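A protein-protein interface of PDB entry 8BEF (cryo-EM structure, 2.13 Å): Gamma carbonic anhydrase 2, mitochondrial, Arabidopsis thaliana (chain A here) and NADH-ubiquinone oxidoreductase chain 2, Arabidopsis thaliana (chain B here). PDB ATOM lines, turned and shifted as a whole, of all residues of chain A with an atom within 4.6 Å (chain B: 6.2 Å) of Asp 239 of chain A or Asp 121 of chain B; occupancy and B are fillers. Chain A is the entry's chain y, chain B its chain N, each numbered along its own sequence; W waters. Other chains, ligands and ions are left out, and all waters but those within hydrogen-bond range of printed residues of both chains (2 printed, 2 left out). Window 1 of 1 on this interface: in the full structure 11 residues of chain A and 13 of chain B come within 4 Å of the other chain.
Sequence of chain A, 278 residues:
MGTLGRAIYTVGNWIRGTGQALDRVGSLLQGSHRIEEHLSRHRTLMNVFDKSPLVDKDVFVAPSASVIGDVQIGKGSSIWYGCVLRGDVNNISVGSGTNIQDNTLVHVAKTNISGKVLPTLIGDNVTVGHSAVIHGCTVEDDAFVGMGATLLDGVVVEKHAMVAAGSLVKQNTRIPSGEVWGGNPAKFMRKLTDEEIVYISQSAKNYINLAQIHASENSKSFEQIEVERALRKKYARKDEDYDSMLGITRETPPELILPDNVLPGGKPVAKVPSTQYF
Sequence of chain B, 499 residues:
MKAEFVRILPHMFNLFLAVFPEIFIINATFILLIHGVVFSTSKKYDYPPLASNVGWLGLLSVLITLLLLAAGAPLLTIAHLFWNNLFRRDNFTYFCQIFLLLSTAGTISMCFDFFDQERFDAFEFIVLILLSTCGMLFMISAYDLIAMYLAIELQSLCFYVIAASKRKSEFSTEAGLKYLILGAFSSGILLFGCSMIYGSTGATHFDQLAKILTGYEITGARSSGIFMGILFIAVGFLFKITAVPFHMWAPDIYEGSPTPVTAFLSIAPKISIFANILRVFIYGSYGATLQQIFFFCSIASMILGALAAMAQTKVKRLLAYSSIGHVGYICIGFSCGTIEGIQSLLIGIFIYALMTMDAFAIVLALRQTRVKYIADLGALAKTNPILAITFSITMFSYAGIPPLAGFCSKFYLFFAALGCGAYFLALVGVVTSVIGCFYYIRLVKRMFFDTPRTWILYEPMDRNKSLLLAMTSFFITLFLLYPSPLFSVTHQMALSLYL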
ATOM      1  N   LYS A 238     -33.770  20.428  -3.535  1.00  0.00           N
ATOM      2  CA  LYS A 238     -32.581  19.592  -3.430  1.00  0.00           C
ATOM      3  C   LYS A 238     -31.786  19.631  -4.727  1.00  0.00           C
ATOM      4  O   LYS A 238     -32.313  19.949  -5.796  1.00  0.00           O
ATOM      5  CB  LYS A 238     -32.945  18.142  -3.083  1.00  0.00           C
ATOM      6  CG  LYS A 238     -34.276  17.681  -3.648  1.00  0.00           C
ATOM      7  CD  LYS A 238     -34.633  16.283  -3.162  1.00  0.00           C
ATOM      8  CE  LYS A 238     -34.986  16.276  -1.684  1.00  0.00           C
ATOM      9  NZ  LYS A 238     -35.563  14.969  -1.263  1.00  0.00           N
ATOM     10  N   ASP A 239     -30.478  19.325  -4.604  1.00  0.00           N
ATOM     11  CA  ASP A 239     -29.609  18.999  -5.743  1.00  0.00           C
ATOM     12  C   ASP A 239     -28.833  17.742  -5.358  1.00  0.00           C
ATOM     13  O   ASP A 239     -27.678  17.809  -4.934  1.00  0.00           O
ATOM     14  CB  ASP A 239     -28.667  20.146  -6.090  1.00  0.00           C
ATOM     15  CG  ASP A 239     -27.890  19.912  -7.381  1.00  0.00           C
ATOM     16  OD1 ASP A 239     -28.053  18.845  -8.012  1.00  0.00           O
ATOM     17  OD2 ASP A 239     -27.118  20.812  -7.773  1.00  0.00           O
ATOM     18  N   GLU A 240     -29.463  16.583  -5.545  1.00  0.00           N
ATOM     19  CA  GLU A 240     -28.829  15.332  -5.150  1.00  0.00           C
ATOM     20  C   GLU A 240     -27.645  14.981  -6.038  1.00  0.00           C
ATOM     21  O   GLU A 240     -26.730  14.288  -5.586  1.00  0.00           O
ATOM     22  CB  GLU A 240     -29.853  14.200  -5.163  1.00  0.00           C
ATOM     23  CG  GLU A 240     -31.034  14.436  -4.242  1.00  0.00           C
ATOM     24  CD  GLU A 240     -31.638  13.143  -3.728  1.00  0.00           C
ATOM     25  OE1 GLU A 240     -32.865  12.963  -3.871  1.00  0.00           O
ATOM     26  OE2 GLU A 240     -30.885  12.310  -3.182  1.00  0.00           O
ATOM     27  N   ASP A 241     -27.638  15.449  -7.285  1.00  0.00           N
ATOM     28  CA  ASP A 241     -26.504  15.194  -8.164  1.00  0.00           C
ATOM     29  C   ASP A 241     -25.243  15.896  -7.668  1.00  0.00           C
ATOM     30  O   ASP A 241     -24.160  15.297  -7.636  1.00  0.00           O
ATOM     31  CB  ASP A 241     -26.849  15.637  -9.581  1.00  0.00           C
ATOM     32  CG  ASP A 241     -25.831  15.185 -10.588  1.00  0.00           C
ATOM     33  OD1 ASP A 241     -25.254  14.093 -10.407  1.00  0.00           O
ATOM     34  OD2 ASP A 241     -25.603  15.930 -11.556  1.00  0.00           O
ATOM     35  N   TYR A 242     -25.363  17.161  -7.262  1.00  0.00           N
ATOM     36  CA  TYR A 242     -24.203  17.855  -6.715  1.00  0.00           C
ATOM     37  C   TYR A 242     -23.789  17.279  -5.370  1.00  0.00           C
ATOM     38  O   TYR A 242     -22.598  17.272  -5.046  1.00  0.00           O
ATOM     39  CB  TYR A 242     -24.474  19.351  -6.581  1.00  0.00           C
ATOM     40  CG  TYR A 242     -23.211  20.182  -6.541  1.00  0.00           C
ATOM     41  CD1 TYR A 242     -22.466  20.396  -7.693  1.00  0.00           C
ATOM     42  CD2 TYR A 242     -22.758  20.737  -5.353  1.00  0.00           C
ATOM     43  CE1 TYR A 242     -21.314  21.151  -7.667  1.00  0.00           C
ATOM     44  CE2 TYR A 242     -21.601  21.498  -5.313  1.00  0.00           C
ATOM     45  CZ  TYR A 242     -20.883  21.701  -6.474  1.00  0.00           C
ATOM     46  OH  TYR A 242     -19.734  22.453  -6.452  1.00  0.00           O
ATOM     47  N   ASP A 243     -24.750  16.804  -4.573  1.00  0.00           N
ATOM     48  CA  ASP A 243     -24.400  16.119  -3.334  1.00  0.00           C
ATOM     49  C   ASP A 243     -23.602  14.852  -3.614  1.00  0.00           C
ATOM     50  O   ASP A 243     -22.619  14.565  -2.926  1.00  0.00           O
ATOM     51  CB  ASP A 243     -25.660  15.790  -2.532  1.00  0.00           C
ATOM     52  CG  ASP A 243     -26.274  17.015  -1.884  1.00  0.00           C
ATOM     53  OD1 ASP A 243     -27.392  17.403  -2.275  1.00  0.00           O
ATOM     54  OD2 ASP A 243     -25.632  17.597  -0.988  1.00  0.00           O
ATOM     55  N   PRO B  48     -22.217  24.377   1.989  1.00  0.00           N
ATOM     56  CA  PRO B  48     -23.231  25.297   1.484  1.00  0.00           C
ATOM     57  C   PRO B  48     -23.217  25.341  -0.030  1.00  0.00           C
ATOM     58  O   PRO B  48     -22.150  25.242  -0.654  1.00  0.00           O
ATOM     59  CB  PRO B  48     -22.811  26.646   2.081  1.00  0.00           C
ATOM     60  CG  PRO B  48     -21.337  26.520   2.257  1.00  0.00           C
ATOM     61  CD  PRO B  48     -21.094  25.087   2.624  1.00  0.00           C
ATOM     62  N   PRO B  49     -24.380  25.463  -0.662  1.00  0.00           N
ATOM     63  CA  PRO B  49     -24.398  25.801  -2.088  1.00  0.00           C
ATOM     64  C   PRO B  49     -23.829  27.197  -2.290  1.00  0.00           C
ATOM     65  O   PRO B  49     -24.166  28.131  -1.564  1.00  0.00           O
ATOM     66  CB  PRO B  49     -25.885  25.734  -2.451  1.00  0.00           C
ATOM     67  CG  PRO B  49     -26.507  24.900  -1.376  1.00  0.00           C
ATOM     68  CD  PRO B  49     -25.733  25.224  -0.136  1.00  0.00           C
ATOM     69  N   LEU B  50     -22.950  27.331  -3.280  1.00  0.00           N
ATOM     70  CA  LEU B  50     -22.276  28.599  -3.528  1.00  0.00           C
ATOM     71  C   LEU B  50     -22.537  29.149  -4.922  1.00  0.00           C
ATOM     72  O   LEU B  50     -21.873  30.109  -5.328  1.00  0.00           O
ATOM     73  CB  LEU B  50     -20.770  28.454  -3.292  1.00  0.00           C
ATOM     74  CG  LEU B  50     -20.377  28.112  -1.855  1.00  0.00           C
ATOM     75  CD1 LEU B  50     -18.867  27.969  -1.723  1.00  0.00           C
ATOM     76  CD2 LEU B  50     -20.920  29.157  -0.889  1.00  0.00           C
ATOM     77  N   ALA B  51     -23.496  28.583  -5.659  1.00  0.00           N
ATOM     78  CA  ALA B  51     -23.761  29.066  -7.008  1.00  0.00           C
ATOM     79  C   ALA B  51     -24.222  30.519  -6.996  1.00  0.00           C
ATOM     80  O   ALA B  51     -23.773  31.320  -7.822  1.00  0.00           O
ATOM     81  CB  ALA B  51     -24.793  28.176  -7.699  1.00  0.00           C
ATOM     82  N   SER B  52     -25.103  30.885  -6.063  1.00  0.00           N
ATOM     83  CA  SER B  52     -25.598  32.258  -6.018  1.00  0.00           C
ATOM     84  C   SER B  52     -24.559  33.226  -5.451  1.00  0.00           C
ATOM     85  O   SER B  52     -24.422  34.347  -5.948  1.00  0.00           O
ATOM     86  CB  SER B  52     -26.899  32.327  -5.216  1.00  0.00           C
ATOM     87  OG  SER B  52     -26.685  32.081  -3.839  1.00  0.00           O
ATOM     88  N   PHE B 115     -30.705  29.116  -9.819  1.00  0.00           N
ATOM     89  CA  PHE B 115     -29.778  28.527  -8.857  1.00  0.00           C
ATOM     90  C   PHE B 115     -30.507  28.048  -7.605  1.00  0.00           C
ATOM     91  O   PHE B 115     -30.310  26.914  -7.159  1.00  0.00           O
ATOM     92  CB  PHE B 115     -28.687  29.528  -8.476  1.00  0.00           C
ATOM     93  CG  PHE B 115     -27.672  29.762  -9.552  1.00  0.00           C
ATOM     94  CD1 PHE B 115     -27.437  28.806 -10.524  1.00  0.00           C
ATOM     95  CD2 PHE B 115     -26.937  30.935  -9.580  1.00  0.00           C
ATOM     96  CE1 PHE B 115     -26.499  29.023 -11.513  1.00  0.00           C
ATOM     97  CE2 PHE B 115     -25.999  31.156 -10.565  1.00  0.00           C
ATOM     98  CZ  PHE B 115     -25.777  30.199 -11.530  1.00  0.00           C
ATOM     99  N   GLU B 118     -34.366  25.554  -8.527  1.00  0.00           N
ATOM    100  CA  GLU B 118     -33.984  24.240  -9.020  1.00  0.00           C
ATOM    101  C   GLU B 118     -33.039  23.558  -8.046  1.00  0.00           C
ATOM    102  O   GLU B 118     -33.013  22.326  -7.959  1.00  0.00           O
ATOM    103  CB  GLU B 118     -33.332  24.370 -10.396  1.00  0.00           C
ATOM    104  CG  GLU B 118     -33.035  23.057 -11.088  1.00  0.00           C
ATOM    105  CD  GLU B 118     -34.114  22.679 -12.079  1.00  0.00           C
ATOM    106  OE1 GLU B 118     -34.949  23.548 -12.404  1.00  0.00           O
ATOM    107  OE2 GLU B 118     -34.128  21.515 -12.534  1.00  0.00           O
ATOM    108  N   ARG B 119     -32.314  24.351  -7.260  1.00  0.00           N
ATOM    109  CA  ARG B 119     -31.093  23.925  -6.592  1.00  0.00           C
ATOM    110  C   ARG B 119     -30.136  23.310  -7.613  1.00  0.00           C
ATOM    111  O   ARG B 119     -29.985  22.103  -7.745  1.00  0.00           O
ATOM    112  CB  ARG B 119     -31.372  23.009  -5.401  1.00  0.00           C
ATOM    113  CG  ARG B 119     -32.087  23.750  -4.297  1.00  0.00           C
ATOM    114  CD  ARG B 119     -31.135  24.307  -3.244  1.00  0.00           C
ATOM    115  NE  ARG B 119     -29.964  23.470  -3.015  1.00  0.00           N
ATOM    116  CZ  ARG B 119     -29.928  22.460  -2.158  1.00  0.00           C
ATOM    117  NH1 ARG B 119     -30.999  22.101  -1.467  1.00  0.00           N
ATOM    118  NH2 ARG B 119     -28.790  21.794  -1.986  1.00  0.00           N
ATOM    119  N   PHE B 120     -29.619  24.207  -8.433  1.00  0.00           N
ATOM    120  CA  PHE B 120     -28.378  23.997  -9.165  1.00  0.00           C
ATOM    121  C   PHE B 120     -27.279  24.629  -8.314  1.00  0.00           C
ATOM    122  O   PHE B 120     -27.087  25.846  -8.342  1.00  0.00           O
ATOM    123  CB  PHE B 120     -28.477  24.619 -10.554  1.00  0.00           C
ATOM    124  CG  PHE B 120     -27.340  24.274 -11.462  1.00  0.00           C
ATOM    125  CD1 PHE B 120     -26.155  24.988 -11.412  1.00  0.00           C
ATOM    126  CD2 PHE B 120     -27.459  23.243 -12.376  1.00  0.00           C
ATOM    127  CE1 PHE B 120     -25.107  24.675 -12.252  1.00  0.00           C
ATOM    128  CE2 PHE B 120     -26.416  22.926 -13.219  1.00  0.00           C
ATOM    129  CZ  PHE B 120     -25.238  23.644 -13.157  1.00  0.00           C
ATOM    130  N   ASP B 121     -26.573  23.811  -7.530  1.00  0.00           N
ATOM    131  CA  ASP B 121     -25.598  24.337  -6.580  1.00  0.00           C
ATOM    132  C   ASP B 121     -24.194  24.492  -7.153  1.00  0.00           C
ATOM    133  O   ASP B 121     -23.320  25.009  -6.453  1.00  0.00           O
ATOM    134  CB  ASP B 121     -25.502  23.462  -5.319  1.00  0.00           C
ATOM    135  CG  ASP B 121     -26.851  23.121  -4.716  1.00  0.00           C
ATOM    136  OD1 ASP B 121     -27.674  24.029  -4.487  1.00  0.00           O
ATOM    137  OD2 ASP B 121     -27.049  21.943  -4.386  1.00  0.00           O
ATOM    138  N   ALA B 122     -23.950  24.062  -8.388  1.00  0.00           N
ATOM    139  CA  ALA B 122     -22.595  24.056  -8.934  1.00  0.00           C
ATOM    140  C   ALA B 122     -22.128  25.482  -9.206  1.00  0.00           C
ATOM    141  O   ALA B 122     -22.613  26.136 -10.133  1.00  0.00           O
ATOM    142  CB  ALA B 122     -22.539  23.214 -10.204  1.00  0.00           C
ATOM    143  N   PHE B 123     -21.185  25.970  -8.396  1.00  0.00           N
ATOM    144  CA  PHE B 123     -20.579  27.270  -8.663  1.00  0.00           C
ATOM    145  C   PHE B 123     -19.657  27.234  -9.874  1.00  0.00           C
ATOM    146  O   PHE B 123     -19.359  28.289 -10.442  1.00  0.00           O
ATOM    147  CB  PHE B 123     -19.795  27.756  -7.443  1.00  0.00           C
ATOM    148  CG  PHE B 123     -18.487  27.047  -7.246  1.00  0.00           C
ATOM    149  CD1 PHE B 123     -17.322  27.529  -7.825  1.00  0.00           C
ATOM    150  CD2 PHE B 123     -18.422  25.893  -6.484  1.00  0.00           C
ATOM    151  CE1 PHE B 123     -16.123  26.873  -7.650  1.00  0.00           C
ATOM    152  CE2 PHE B 123     -17.225  25.234  -6.306  1.00  0.00           C
ATOM    153  CZ  PHE B 123     -16.075  25.720  -6.890  1.00  0.00           C
ATOM    154  N   GLU B 124     -19.180  26.048 -10.262  1.00  0.00           N
ATOM    155  CA  GLU B 124     -18.292  25.938 -11.414  1.00  0.00           C
ATOM    156  C   GLU B 124     -18.960  26.447 -12.683  1.00  0.00           C
ATOM    157  O   GLU B 124     -18.276  26.846 -13.629  1.00  0.00           O
ATOM    158  CB  GLU B 124     -17.842  24.487 -11.589  1.00  0.00           C
ATOM    159  CG  GLU B 124     -16.888  23.997 -10.505  1.00  0.00           C
ATOM    160  CD  GLU B 124     -17.602  23.351  -9.323  1.00  0.00           C
ATOM    161  OE1 GLU B 124     -18.779  23.680  -9.073  1.00  0.00           O
ATOM    162  OE2 GLU B 124     -16.975  22.517  -8.639  1.00  0.00           O
ATOM    163  N   LYS B 166     -26.348  19.586 -16.564  1.00  0.00           N
ATOM    164  CA  LYS B 166     -27.327  18.654 -15.934  1.00  0.00           C
ATOM    165  C   LYS B 166     -26.844  17.275 -16.376  1.00  0.00           C
ATOM    166  O   LYS B 166     -27.382  16.739 -17.357  1.00  0.00           O
ATOM    167  CB  LYS B 166     -28.767  19.011 -16.315  1.00  0.00           C
ATOM    168  CG  LYS B 166     -29.246  20.358 -15.787  1.00  0.00           C
ATOM    169  CD  LYS B 166     -30.505  20.275 -14.951  1.00  0.00           C
ATOM    170  CE  LYS B 166     -30.316  19.516 -13.656  1.00  0.00           C
ATOM    171  NZ  LYS B 166     -31.556  19.502 -12.843  1.00  0.00           N
HETATM  172  O   HOH W   1     -25.403  21.757 -10.197  1.00  0.00           O
HETATM  173  O   HOH W   2     -29.567  18.953  -2.321  1.00  0.00           O
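The side-chain carboxylate (OD2) of Asp 239 of chain A is in hydrogen-bond range of the backbone NH (N) of Asp 121 of chain B (3.1 Å).
OH of Tyr 242 of chain A sits at hydrogen-bond distance from OE1 of Glu 124 of chain B (3.0 Å).
The backbone carbonyl oxygen of Lys 238 of chain A sits close to the backbone carbonyl oxygen of Glu 118 of chain B, at 3.3 Å.
O of Arg 119 of chain B sits close to OD2 of Asp 239 of chain A (3.1 Å).
The side-chain carboxylate of Asp 239 of chain A lies close to the backbone NH of Asp 241 of chain A (3.5 Å).
The side-chain carboxylate (OD1) of Asp 239 of chain A lies within hydrogen-bond range of the backbone NH (N) of Tyr 242 of chain A, 3.3 Å away.
The backbone carbonyl oxygen (O) of Asp 239 of chain A sits close to the side-chain carboxylate (OD1) of Asp 243 of chain A, at 2.7 Å.
The backbone carbonyl oxygen of Phe 115 of chain B is in hydrogen-bond range of the backbone NH of Phe 120 of chain B (3.1 Å).
NZ of Lys 166 of chain B is in salt-bridge range of OE2 of Glu 118 of chain B (3.3 Å).
The guanidinium group (NE) of Arg 119 of chain B lies within salt-bridge range of the side-chain carboxylate (OD1) of Asp 121 of chain B (2.8 Å).
Among the printed residues, pairs that only touch across the chains: Lys 238 of chain A with Arg 119 of chain B (3.2 Å), Asp 239 of chain A with Phe 120 of chain B (3.7 Å), Tyr 242 of chain A with Asp 121 of chain B (3.9 Å), Tyr 242 of chain A with Ala 122 of chain B (3.4 Å) and Tyr 242 of chain A with Phe 123 of chain B (3.7 Å).
Asp 239 of chain A touches three residues of chain B.
Asp 121 of chain B touches just these residues of chain A: Asp 239 and Tyr 242.
Printed residues of chain B within 4 Å of Lys 238 of chain A: Glu 118 and Arg 119.
Of the printed residues of chain A, Phe 120 of chain B touches Asp 239.
Printed residues of chain B within 4 Å of Tyr 242 of chain A: Asp 121 (3.9 Å), Ala 122 (3.4 Å), Phe 123 (3.7 Å) and Glu 124 (3.0 Å).
Printed residues of chain A within 4 Å of Glu 118 of chain B: Lys 238 (3.3 Å).
Asp 241 of chain A touches none of the printed residues of chain B.
The nearest residue of chain B that does not touch Asp 239 of chain A is Ala 122 of chain B (4.6 Å).
The nearest printed residue of chain A that does not touch Asp 121 of chain B is Asp 243 of chain A (5.0 Å).
Of the 14 printed residues of chain B, 7 touch a printed residue of chain A.
Hydrophobic or aromatic side chains of chain B within 4 Å of the printed part of chain A: Ala 122 and Phe 123.
Of the 6 printed residues of chain A, 3 touch a printed residue of chain B.
Hydrophobic or aromatic side chains of chain A within 4 Å of the printed part of chain B: Tyr 242.
Among the printed residues, no Asp or Glu carboxylate lies within 4 Å of a Lys or Arg side-chain nitrogen of the other chain.
Water W2 lies within hydrogen-bond range of N of Asp 239 of chain A (2.5 Å), OD1 of Asp 243 of chain A (2.7 Å) and NH2 of Arg 119 of chain B (3.0 Å).
Water W1 bridges the side-chain carboxylate of Asp 239 of chain A and the backbone NH of Ala 122 of chain B.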
